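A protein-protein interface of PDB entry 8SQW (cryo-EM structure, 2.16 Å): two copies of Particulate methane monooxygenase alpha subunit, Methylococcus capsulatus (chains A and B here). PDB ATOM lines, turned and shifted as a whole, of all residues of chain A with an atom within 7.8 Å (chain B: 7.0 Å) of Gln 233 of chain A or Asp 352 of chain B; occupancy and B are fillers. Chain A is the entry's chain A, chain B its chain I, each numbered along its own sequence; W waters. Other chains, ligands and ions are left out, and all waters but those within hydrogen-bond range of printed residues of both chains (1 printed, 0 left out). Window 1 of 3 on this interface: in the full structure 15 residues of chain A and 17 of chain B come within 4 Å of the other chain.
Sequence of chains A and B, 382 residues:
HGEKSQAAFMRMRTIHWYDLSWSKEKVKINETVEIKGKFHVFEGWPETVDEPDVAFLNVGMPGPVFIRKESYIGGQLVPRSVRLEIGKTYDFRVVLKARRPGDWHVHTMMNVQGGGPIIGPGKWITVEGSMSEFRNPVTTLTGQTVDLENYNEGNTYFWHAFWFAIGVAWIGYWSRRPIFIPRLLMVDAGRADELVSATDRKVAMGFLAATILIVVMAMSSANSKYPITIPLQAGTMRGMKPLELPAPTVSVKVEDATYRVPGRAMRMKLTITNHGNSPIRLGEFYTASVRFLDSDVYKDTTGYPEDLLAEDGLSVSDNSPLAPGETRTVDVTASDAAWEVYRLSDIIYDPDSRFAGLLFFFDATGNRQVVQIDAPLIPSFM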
ATOM      1  N   PRO A  79     -28.332   2.985  -8.837  1.00  0.00           N
ATOM      2  CA  PRO A  79     -29.174   3.802  -7.953  1.00  0.00           C
ATOM      3  C   PRO A  79     -28.423   4.393  -6.775  1.00  0.00           C
ATOM      4  O   PRO A  79     -28.983   5.246  -6.074  1.00  0.00           O
ATOM      5  CB  PRO A  79     -30.246   2.813  -7.484  1.00  0.00           C
ATOM      6  CG  PRO A  79     -29.548   1.502  -7.493  1.00  0.00           C
ATOM      7  CD  PRO A  79     -28.558   1.544  -8.632  1.00  0.00           C
ATOM      8  N   ARG A  80     -27.191   3.968  -6.531  1.00  0.00           N
ATOM      9  CA  ARG A  80     -26.374   4.455  -5.434  1.00  0.00           C
ATOM     10  C   ARG A  80     -25.151   5.179  -5.989  1.00  0.00           C
ATOM     11  O   ARG A  80     -24.942   5.262  -7.201  1.00  0.00           O
ATOM     12  CB  ARG A  80     -25.963   3.302  -4.520  1.00  0.00           C
ATOM     13  CG  ARG A  80     -27.066   2.285  -4.270  1.00  0.00           C
ATOM     14  CD  ARG A  80     -26.876   1.589  -2.942  1.00  0.00           C
ATOM     15  NE  ARG A  80     -27.258   0.182  -2.989  1.00  0.00           N
ATOM     16  CZ  ARG A  80     -26.442  -0.822  -2.701  1.00  0.00           C
ATOM     17  NH1 ARG A  80     -25.183  -0.613  -2.361  1.00  0.00           N
ATOM     18  NH2 ARG A  80     -26.905  -2.066  -2.749  1.00  0.00           N
ATOM     19  N   ILE A 230     -37.290  -4.247   4.882  1.00  0.00           N
ATOM     20  CA  ILE A 230     -35.838  -4.233   4.735  1.00  0.00           C
ATOM     21  C   ILE A 230     -35.339  -2.830   5.058  1.00  0.00           C
ATOM     22  O   ILE A 230     -36.081  -1.855   4.880  1.00  0.00           O
ATOM     23  CB  ILE A 230     -35.411  -4.665   3.323  1.00  0.00           C
ATOM     24  CG1 ILE A 230     -36.061  -3.769   2.268  1.00  0.00           C
ATOM     25  CG2 ILE A 230     -35.755  -6.126   3.078  1.00  0.00           C
ATOM     26  CD1 ILE A 230     -35.258  -3.651   0.996  1.00  0.00           C
ATOM     27  N   PRO A 231     -34.108  -2.677   5.536  1.00  0.00           N
ATOM     28  CA  PRO A 231     -33.571  -1.334   5.766  1.00  0.00           C
ATOM     29  C   PRO A 231     -33.300  -0.622   4.451  1.00  0.00           C
ATOM     30  O   PRO A 231     -33.340  -1.206   3.367  1.00  0.00           O
ATOM     31  CB  PRO A 231     -32.275  -1.592   6.539  1.00  0.00           C
ATOM     32  CG  PRO A 231     -31.873  -2.964   6.131  1.00  0.00           C
ATOM     33  CD  PRO A 231     -33.149  -3.727   5.916  1.00  0.00           C
ATOM     34  N   LEU A 232     -33.028   0.676   4.563  1.00  0.00           N
ATOM     35  CA  LEU A 232     -32.658   1.464   3.397  1.00  0.00           C
ATOM     36  C   LEU A 232     -31.392   0.898   2.768  1.00  0.00           C
ATOM     37  O   LEU A 232     -30.416   0.600   3.463  1.00  0.00           O
ATOM     38  CB  LEU A 232     -32.449   2.924   3.794  1.00  0.00           C
ATOM     39  CG  LEU A 232     -33.697   3.648   4.295  1.00  0.00           C
ATOM     40  CD1 LEU A 232     -33.336   5.006   4.867  1.00  0.00           C
ATOM     41  CD2 LEU A 232     -34.708   3.789   3.175  1.00  0.00           C
ATOM     42  N   GLN A 233     -31.409   0.746   1.448  1.00  0.00           N
ATOM     43  CA  GLN A 233     -30.287   0.174   0.720  1.00  0.00           C
ATOM     44  C   GLN A 233     -29.339   1.292   0.301  1.00  0.00           C
ATOM     45  O   GLN A 233     -29.703   2.150  -0.508  1.00  0.00           O
ATOM     46  CB  GLN A 233     -30.777  -0.610  -0.496  1.00  0.00           C
ATOM     47  CG  GLN A 233     -31.681  -1.782  -0.151  1.00  0.00           C
ATOM     48  CD  GLN A 233     -30.978  -2.847   0.667  1.00  0.00           C
ATOM     49  OE1 GLN A 233     -30.261  -3.687   0.127  1.00  0.00           O
ATOM     50  NE2 GLN A 233     -31.185  -2.820   1.978  1.00  0.00           N
ATOM     51  N   ALA A 234     -28.127   1.275   0.851  1.00  0.00           N
ATOM     52  CA  ALA A 234     -27.158   2.328   0.600  1.00  0.00           C
ATOM     53  C   ALA A 234     -25.772   1.712   0.487  1.00  0.00           C
ATOM     54  O   ALA A 234     -25.558   0.543   0.814  1.00  0.00           O
ATOM     55  CB  ALA A 234     -27.195   3.393   1.699  1.00  0.00           C
ATOM     56  N   GLY A 235     -24.830   2.517   0.004  1.00  0.00           N
ATOM     57  CA  GLY A 235     -23.452   2.083  -0.118  1.00  0.00           C
ATOM     58  C   GLY A 235     -22.873   2.324  -1.497  1.00  0.00           C
ATOM     59  O   GLY A 235     -23.494   1.970  -2.505  1.00  0.00           O
ATOM     60  N   THR A 236     -21.691   2.933  -1.552  1.00  0.00           N
ATOM     61  CA  THR A 236     -21.034   3.180  -2.829  1.00  0.00           C
ATOM     62  C   THR A 236     -20.758   1.866  -3.547  1.00  0.00           C
ATOM     63  O   THR A 236     -20.351   0.875  -2.933  1.00  0.00           O
ATOM     64  CB  THR A 236     -19.731   3.953  -2.616  1.00  0.00           C
ATOM     65  OG1 THR A 236     -20.012   5.188  -1.945  1.00  0.00           O
ATOM     66  CG2 THR A 236     -19.054   4.254  -3.945  1.00  0.00           C
ATOM     67  N   MET A 237     -20.989   1.859  -4.855  1.00  0.00           N
ATOM     68  CA  MET A 237     -20.849   0.663  -5.672  1.00  0.00           C
ATOM     69  C   MET A 237     -19.542   0.743  -6.450  1.00  0.00           C
ATOM     70  O   MET A 237     -19.320   1.695  -7.206  1.00  0.00           O
ATOM     71  CB  MET A 237     -22.038   0.522  -6.617  1.00  0.00           C
ATOM     72  CG  MET A 237     -23.310   0.066  -5.921  1.00  0.00           C
ATOM     73  SD  MET A 237     -24.770   0.206  -6.964  1.00  0.00           S
ATOM     74  CE  MET A 237     -24.229  -0.704  -8.401  1.00  0.00           C
ATOM     75  N   ALA B   8     -23.793 -10.223   6.807  1.00  0.00           N
ATOM     76  CA  ALA B   8     -23.585 -11.287   5.832  1.00  0.00           C
ATOM     77  C   ALA B   8     -22.936 -10.759   4.560  1.00  0.00           C
ATOM     78  O   ALA B   8     -22.016 -11.384   4.021  1.00  0.00           O
ATOM     79  CB  ALA B   8     -24.913 -11.973   5.513  1.00  0.00           C
ATOM     80  N   PHE B   9     -23.394  -9.606   4.067  1.00  0.00           N
ATOM     81  CA  PHE B   9     -22.829  -9.076   2.829  1.00  0.00           C
ATOM     82  C   PHE B   9     -21.396  -8.609   3.036  1.00  0.00           C
ATOM     83  O   PHE B   9     -20.574  -8.677   2.114  1.00  0.00           O
ATOM     84  CB  PHE B   9     -23.709  -7.952   2.283  1.00  0.00           C
ATOM     85  CG  PHE B   9     -23.421  -6.593   2.866  1.00  0.00           C
ATOM     86  CD1 PHE B   9     -24.018  -6.193   4.048  1.00  0.00           C
ATOM     87  CD2 PHE B   9     -22.591  -5.698   2.210  1.00  0.00           C
ATOM     88  CE1 PHE B   9     -23.775  -4.940   4.580  1.00  0.00           C
ATOM     89  CE2 PHE B   9     -22.340  -4.446   2.736  1.00  0.00           C
ATOM     90  CZ  PHE B   9     -22.938  -4.065   3.920  1.00  0.00           C
ATOM     91  N   MET B  10     -21.068  -8.142   4.241  1.00  0.00           N
ATOM     92  CA  MET B  10     -19.700  -7.722   4.507  1.00  0.00           C
ATOM     93  C   MET B  10     -18.774  -8.925   4.624  1.00  0.00           C
ATOM     94  O   MET B  10     -17.615  -8.867   4.198  1.00  0.00           O
ATOM     95  CB  MET B  10     -19.651  -6.876   5.777  1.00  0.00           C
ATOM     96  CG  MET B  10     -20.604  -5.707   5.714  1.00  0.00           C
ATOM     97  SD  MET B  10     -19.817  -4.121   5.418  1.00  0.00           S
ATOM     98  CE  MET B  10     -18.570  -4.154   6.681  1.00  0.00           C
ATOM     99  N   ARG B  13     -18.326 -10.005   0.841  1.00  0.00           N
ATOM    100  CA  ARG B  13     -17.474  -9.166   0.012  1.00  0.00           C
ATOM    101  C   ARG B  13     -16.505  -8.380   0.889  1.00  0.00           C
ATOM    102  O   ARG B  13     -16.634  -7.169   1.060  1.00  0.00           O
ATOM    103  CB  ARG B  13     -18.355  -8.217  -0.809  1.00  0.00           C
ATOM    104  CG  ARG B  13     -19.736  -8.760  -1.130  1.00  0.00           C
ATOM    105  CD  ARG B  13     -20.773  -7.650  -1.243  1.00  0.00           C
ATOM    106  NE  ARG B  13     -20.380  -6.600  -2.173  1.00  0.00           N
ATOM    107  CZ  ARG B  13     -20.532  -6.666  -3.489  1.00  0.00           C
ATOM    108  NH1 ARG B  13     -21.065  -7.726  -4.071  1.00  0.00           N
ATOM    109  NH2 ARG B  13     -20.141  -5.641  -4.237  1.00  0.00           N
ATOM    110  N   PRO B  46     -16.413  -2.896   0.244  1.00  0.00           N
ATOM    111  CA  PRO B  46     -17.466  -1.986   0.715  1.00  0.00           C
ATOM    112  C   PRO B  46     -16.890  -0.639   1.131  1.00  0.00           C
ATOM    113  O   PRO B  46     -15.816  -0.563   1.730  1.00  0.00           O
ATOM    114  CB  PRO B  46     -18.081  -2.735   1.901  1.00  0.00           C
ATOM    115  CG  PRO B  46     -17.033  -3.703   2.331  1.00  0.00           C
ATOM    116  CD  PRO B  46     -16.274  -4.084   1.102  1.00  0.00           C
ATOM    117  N   GLU B  47     -17.622   0.427   0.805  1.00  0.00           N
ATOM    118  CA  GLU B  47     -17.152   1.772   1.119  1.00  0.00           C
ATOM    119  C   GLU B  47     -17.091   2.025   2.617  1.00  0.00           C
ATOM    120  O   GLU B  47     -16.310   2.872   3.063  1.00  0.00           O
ATOM    121  CB  GLU B  47     -18.050   2.813   0.449  1.00  0.00           C
ATOM    122  CG  GLU B  47     -19.388   3.028   1.136  1.00  0.00           C
ATOM    123  CD  GLU B  47     -19.864   4.464   1.044  1.00  0.00           C
ATOM    124  OE1 GLU B  47     -19.011   5.374   1.021  1.00  0.00           O
ATOM    125  OE2 GLU B  47     -21.092   4.682   0.989  1.00  0.00           O
ATOM    126  N   ILE B 347     -28.818 -11.690   5.501  1.00  0.00           N
ATOM    127  CA  ILE B 347     -28.503 -10.573   4.561  1.00  0.00           C
ATOM    128  C   ILE B 347     -29.802  -9.783   4.336  1.00  0.00           C
ATOM    129  O   ILE B 347     -29.727  -8.649   3.823  1.00  0.00           O
ATOM    130  CB  ILE B 347     -27.857 -11.114   3.264  1.00  0.00           C
ATOM    131  CG1 ILE B 347     -27.311  -9.998   2.365  1.00  0.00           C
ATOM    132  CG2 ILE B 347     -28.809 -12.032   2.518  1.00  0.00           C
ATOM    133  CD1 ILE B 347     -26.481 -10.487   1.207  1.00  0.00           C
ATOM    134  N   ILE B 348     -30.950 -10.333   4.749  1.00  0.00           N
ATOM    135  CA  ILE B 348     -32.187  -9.566   4.639  1.00  0.00           C
ATOM    136  C   ILE B 348     -32.178  -8.386   5.605  1.00  0.00           C
ATOM    137  O   ILE B 348     -32.857  -7.379   5.370  1.00  0.00           O
ATOM    138  CB  ILE B 348     -33.401 -10.486   4.866  1.00  0.00           C
ATOM    139  CG1 ILE B 348     -34.685  -9.817   4.367  1.00  0.00           C
ATOM    140  CG2 ILE B 348     -33.519 -10.885   6.332  1.00  0.00           C
ATOM    141  CD1 ILE B 348     -35.942 -10.517   4.809  1.00  0.00           C
ATOM    142  N   TYR B 349     -31.419  -8.483   6.694  1.00  0.00           N
ATOM    143  CA  TYR B 349     -31.262  -7.379   7.631  1.00  0.00           C
ATOM    144  C   TYR B 349     -30.234  -6.357   7.166  1.00  0.00           C
ATOM    145  O   TYR B 349     -30.210  -5.239   7.690  1.00  0.00           O
ATOM    146  CB  TYR B 349     -30.871  -7.926   9.009  1.00  0.00           C
ATOM    147  CG  TYR B 349     -30.776  -6.887  10.104  1.00  0.00           C
ATOM    148  CD1 TYR B 349     -31.903  -6.491  10.808  1.00  0.00           C
ATOM    149  CD2 TYR B 349     -29.559  -6.304  10.434  1.00  0.00           C
ATOM    150  CE1 TYR B 349     -31.823  -5.544  11.808  1.00  0.00           C
ATOM    151  CE2 TYR B 349     -29.470  -5.355  11.431  1.00  0.00           C
ATOM    152  CZ  TYR B 349     -30.605  -4.977  12.112  1.00  0.00           C
ATOM    153  OH  TYR B 349     -30.522  -4.036  13.108  1.00  0.00           O
ATOM    154  N   ASP B 350     -29.408  -6.698   6.187  1.00  0.00           N
ATOM    155  CA  ASP B 350     -28.309  -5.844   5.781  1.00  0.00           C
ATOM    156  C   ASP B 350     -28.792  -4.675   4.924  1.00  0.00           C
ATOM    157  O   ASP B 350     -29.769  -4.802   4.183  1.00  0.00           O
ATOM    158  CB  ASP B 350     -27.275  -6.652   5.007  1.00  0.00           C
ATOM    159  CG  ASP B 350     -26.469  -7.576   5.899  1.00  0.00           C
ATOM    160  OD1 ASP B 350     -26.345  -7.278   7.106  1.00  0.00           O
ATOM    161  OD2 ASP B 350     -25.959  -8.598   5.395  1.00  0.00           O
ATOM    162  N   PRO B 351     -28.117  -3.529   5.009  1.00  0.00           N
ATOM    163  CA  PRO B 351     -28.448  -2.393   4.143  1.00  0.00           C
ATOM    164  C   PRO B 351     -27.846  -2.466   2.749  1.00  0.00           C
ATOM    165  O   PRO B 351     -27.932  -1.479   2.009  1.00  0.00           O
ATOM    166  CB  PRO B 351     -27.866  -1.204   4.921  1.00  0.00           C
ATOM    167  CG  PRO B 351     -26.697  -1.778   5.626  1.00  0.00           C
ATOM    168  CD  PRO B 351     -27.076  -3.188   5.994  1.00  0.00           C
ATOM    169  N   ASP B 352     -27.229  -3.586   2.375  1.00  0.00           N
ATOM    170  CA  ASP B 352     -26.662  -3.747   1.037  1.00  0.00           C
ATOM    171  C   ASP B 352     -26.794  -5.223   0.672  1.00  0.00           C
ATOM    172  O   ASP B 352     -25.932  -6.030   1.031  1.00  0.00           O
ATOM    173  CB  ASP B 352     -25.212  -3.284   0.991  1.00  0.00           C
ATOM    174  CG  ASP B 352     -24.686  -3.147  -0.424  1.00  0.00           C
ATOM    175  OD1 ASP B 352     -25.412  -3.505  -1.374  1.00  0.00           O
ATOM    176  OD2 ASP B 352     -23.540  -2.680  -0.587  1.00  0.00           O
ATOM    177  N   SER B 353     -27.864  -5.563  -0.045  1.00  0.00           N
ATOM    178  CA  SER B 353     -28.155  -6.956  -0.384  1.00  0.00           C
ATOM    179  C   SER B 353     -27.434  -7.334  -1.679  1.00  0.00           C
ATOM    180  O   SER B 353     -28.032  -7.533  -2.739  1.00  0.00           O
ATOM    181  CB  SER B 353     -29.656  -7.175  -0.498  1.00  0.00           C
ATOM    182  OG  SER B 353     -29.984  -8.540  -0.294  1.00  0.00           O
ATOM    183  N   ARG B 354     -26.114  -7.432  -1.568  1.00  0.00           N
ATOM    184  CA  ARG B 354     -25.272  -7.902  -2.652  1.00  0.00           C
ATOM    185  C   ARG B 354     -24.335  -8.972  -2.114  1.00  0.00           C
ATOM    186  O   ARG B 354     -23.817  -8.862  -1.000  1.00  0.00           O
ATOM    187  CB  ARG B 354     -24.465  -6.761  -3.283  1.00  0.00           C
ATOM    188  CG  ARG B 354     -25.300  -5.805  -4.118  1.00  0.00           C
ATOM    189  CD  ARG B 354     -24.441  -4.738  -4.770  1.00  0.00           C
ATOM    190  NE  ARG B 354     -23.739  -3.926  -3.784  1.00  0.00           N
ATOM    191  CZ  ARG B 354     -22.698  -3.150  -4.060  1.00  0.00           C
ATOM    192  NH1 ARG B 354     -22.214  -3.053  -5.285  1.00  0.00           N
ATOM    193  NH2 ARG B 354     -22.129  -2.454  -3.078  1.00  0.00           N
ATOM    194  N   PHE B 355     -24.134 -10.016  -2.908  1.00  0.00           N
ATOM    195  CA  PHE B 355     -23.269 -11.117  -2.526  1.00  0.00           C
ATOM    196  C   PHE B 355     -22.056 -11.164  -3.443  1.00  0.00           C
ATOM    197  O   PHE B 355     -22.064 -10.622  -4.550  1.00  0.00           O
ATOM    198  CB  PHE B 355     -24.016 -12.461  -2.571  1.00  0.00           C
ATOM    199  CG  PHE B 355     -23.950 -13.148  -3.906  1.00  0.00           C
ATOM    200  CD1 PHE B 355     -24.850 -12.826  -4.908  1.00  0.00           C
ATOM    201  CD2 PHE B 355     -23.000 -14.127  -4.157  1.00  0.00           C
ATOM    202  CE1 PHE B 355     -24.795 -13.454  -6.136  1.00  0.00           C
ATOM    203  CE2 PHE B 355     -22.938 -14.756  -5.386  1.00  0.00           C
ATOM    204  CZ  PHE B 355     -23.841 -14.422  -6.375  1.00  0.00           C
ATOM    205  N   LEU B 377     -28.470  -9.823  -4.414  1.00  0.00           N
ATOM    206  CA  LEU B 377     -29.113 -11.023  -3.889  1.00  0.00           C
ATOM    207  C   LEU B 377     -30.527 -10.638  -3.466  1.00  0.00           C
ATOM    208  O   LEU B 377     -30.711  -9.912  -2.483  1.00  0.00           O
ATOM    209  CB  LEU B 377     -28.311 -11.600  -2.726  1.00  0.00           C
ATOM    210  CG  LEU B 377     -28.725 -12.976  -2.207  1.00  0.00           C
ATOM    211  CD1 LEU B 377     -28.469 -14.045  -3.254  1.00  0.00           C
ATOM    212  CD2 LEU B 377     -27.992 -13.299  -0.913  1.00  0.00           C
HETATM  213  O   HOH W   1     -20.185  -0.622  -0.620  1.00  0.00           O
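The backbone carbonyl oxygen of Ala 234 of chain A is in hydrogen-bond range of the guanidinium group of Arg 80 of chain A (3.4 Å).
O of Gly 235 of chain A sits at hydrogen-bond distance from NH1 of Arg 80 of chain A (3.1 Å).
O of Pro 231 of chain A sits at hydrogen-bond distance from NE2 of Gln 233 of chain A (3.0 Å).
The side-chain carboxylate (OD2) of Asp 350 of chain B sits at hydrogen-bond distance from the backbone NH (N) of Phe 9 of chain B.
OG of Ser 353 of chain B is in hydrogen-bond range of O of Leu 377 of chain B (2.7 Å).
N of Ala 8 of chain B is in hydrogen-bond range of OD2 of Asp 350 of chain B, 3.1 Å away.
The guanidinium group (NH2) of Arg 80 of chain A is in salt-bridge range of the side-chain carboxylate (OD1) of Asp 352 of chain B, 2.5 Å away.
OE1 of Gln 233 of chain A lies within hydrogen-bond range of N of Ser 353 of chain B.
The backbone NH of Ala 234 of chain A lies within hydrogen-bond range of the backbone carbonyl oxygen of Pro 351 of chain B (3.0 Å).
NE2 of Gln 233 of chain A is in hydrogen-bond range of O of Asp 350 of chain B, at 3.3 Å.
The side-chain carboxylate (OE1) of Glu 47 of chain B sits close to the side-chain hydroxyl (OG1) of Thr 236 of chain A (3.1 Å).
Water W1 lies within hydrogen-bond range of the backbone carbonyl oxygen (O) of Thr 236 of chain A (2.8 Å) and the backbone NH (N) of Glu 47 of chain B (3.1 Å).
No position is printed for both chains.
Of the 18 pairs that touch across the chains among the printed residues, none has its exchanged pair printed and touching as well.
Arg 80 of chain A touches Arg 354 of chain B.
CG2 of Ile 230 of chain A touches O of Ile 348 of chain B (3.9 Å).
Pro 231 of chain A touches Ile 348 of chain B.
CG of Pro 231 of chain A touches O of Tyr 349 of chain B, at 3.2 Å.
Pro 351 of chain B touches Pro 231 of chain A (N to CG, 3.96 Å).
Leu 232 of chain A touches Pro 351 of chain B (O to CB, 3.4 Å).
Ala 234 of chain A touches Asp 352 of chain B (O to CB, 3.8 Å).
Gly 235 of chain A touches Glu 47 of chain B (CA to OE2, 3.7 Å).
Thr 236 of chain A touches Arg 354 of chain B.
Met 237 of chain A touches Arg 354 of chain B.
Of the printed residues of chain B, Gln 233 of chain A touches Asp 350 (3.3 Å), Pro 351 (3.2 Å), Asp 352 (3.7 Å) and Ser 353 (3.0 Å).
Asp 352 of chain B touches three residues of chain A.
Of the printed residues of chain B, Ala 234 of chain A touches Pro 351 (3.0 Å) and Asp 352 (3.8 Å).
Printed residues of chain B within 4 Å of Ile 230 of chain A: Ile 348.
Printed residues of chain B within 4 Å of Met 237 of chain A: Arg 354 (3.4 Å).
Printed residues of chain B within 4 Å of Thr 236 of chain A: Glu 47 (3.1 Å) and Arg 354 (3.8 Å).
Pro 79 of chain A touches none of the printed residues of chain B.
Ile 347 of chain B touches none of the printed residues of chain A.
The nearest residue of chain B that does not touch Gln 233 of chain A is Arg 354 of chain B (5.8 Å).
Of the 16 printed residues of chain B, 8 touch a printed residue of chain A.
Along chain B the printed residues that touch a printed residue of chain A span positions 47 to 354.
Of the 10 printed residues of chain A, 9 touch a printed residue of chain B.
Hydrophobic or aromatic side chains of chain A within 4 Å of the printed part of chain B: Ile 230, Pro 231 and Met 237.
Among the printed residues, Asp or Glu carboxylates within 4 Å of a Lys or Arg side-chain nitrogen of the other chain: Arg 80 of chain A with Asp 352 of chain B.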
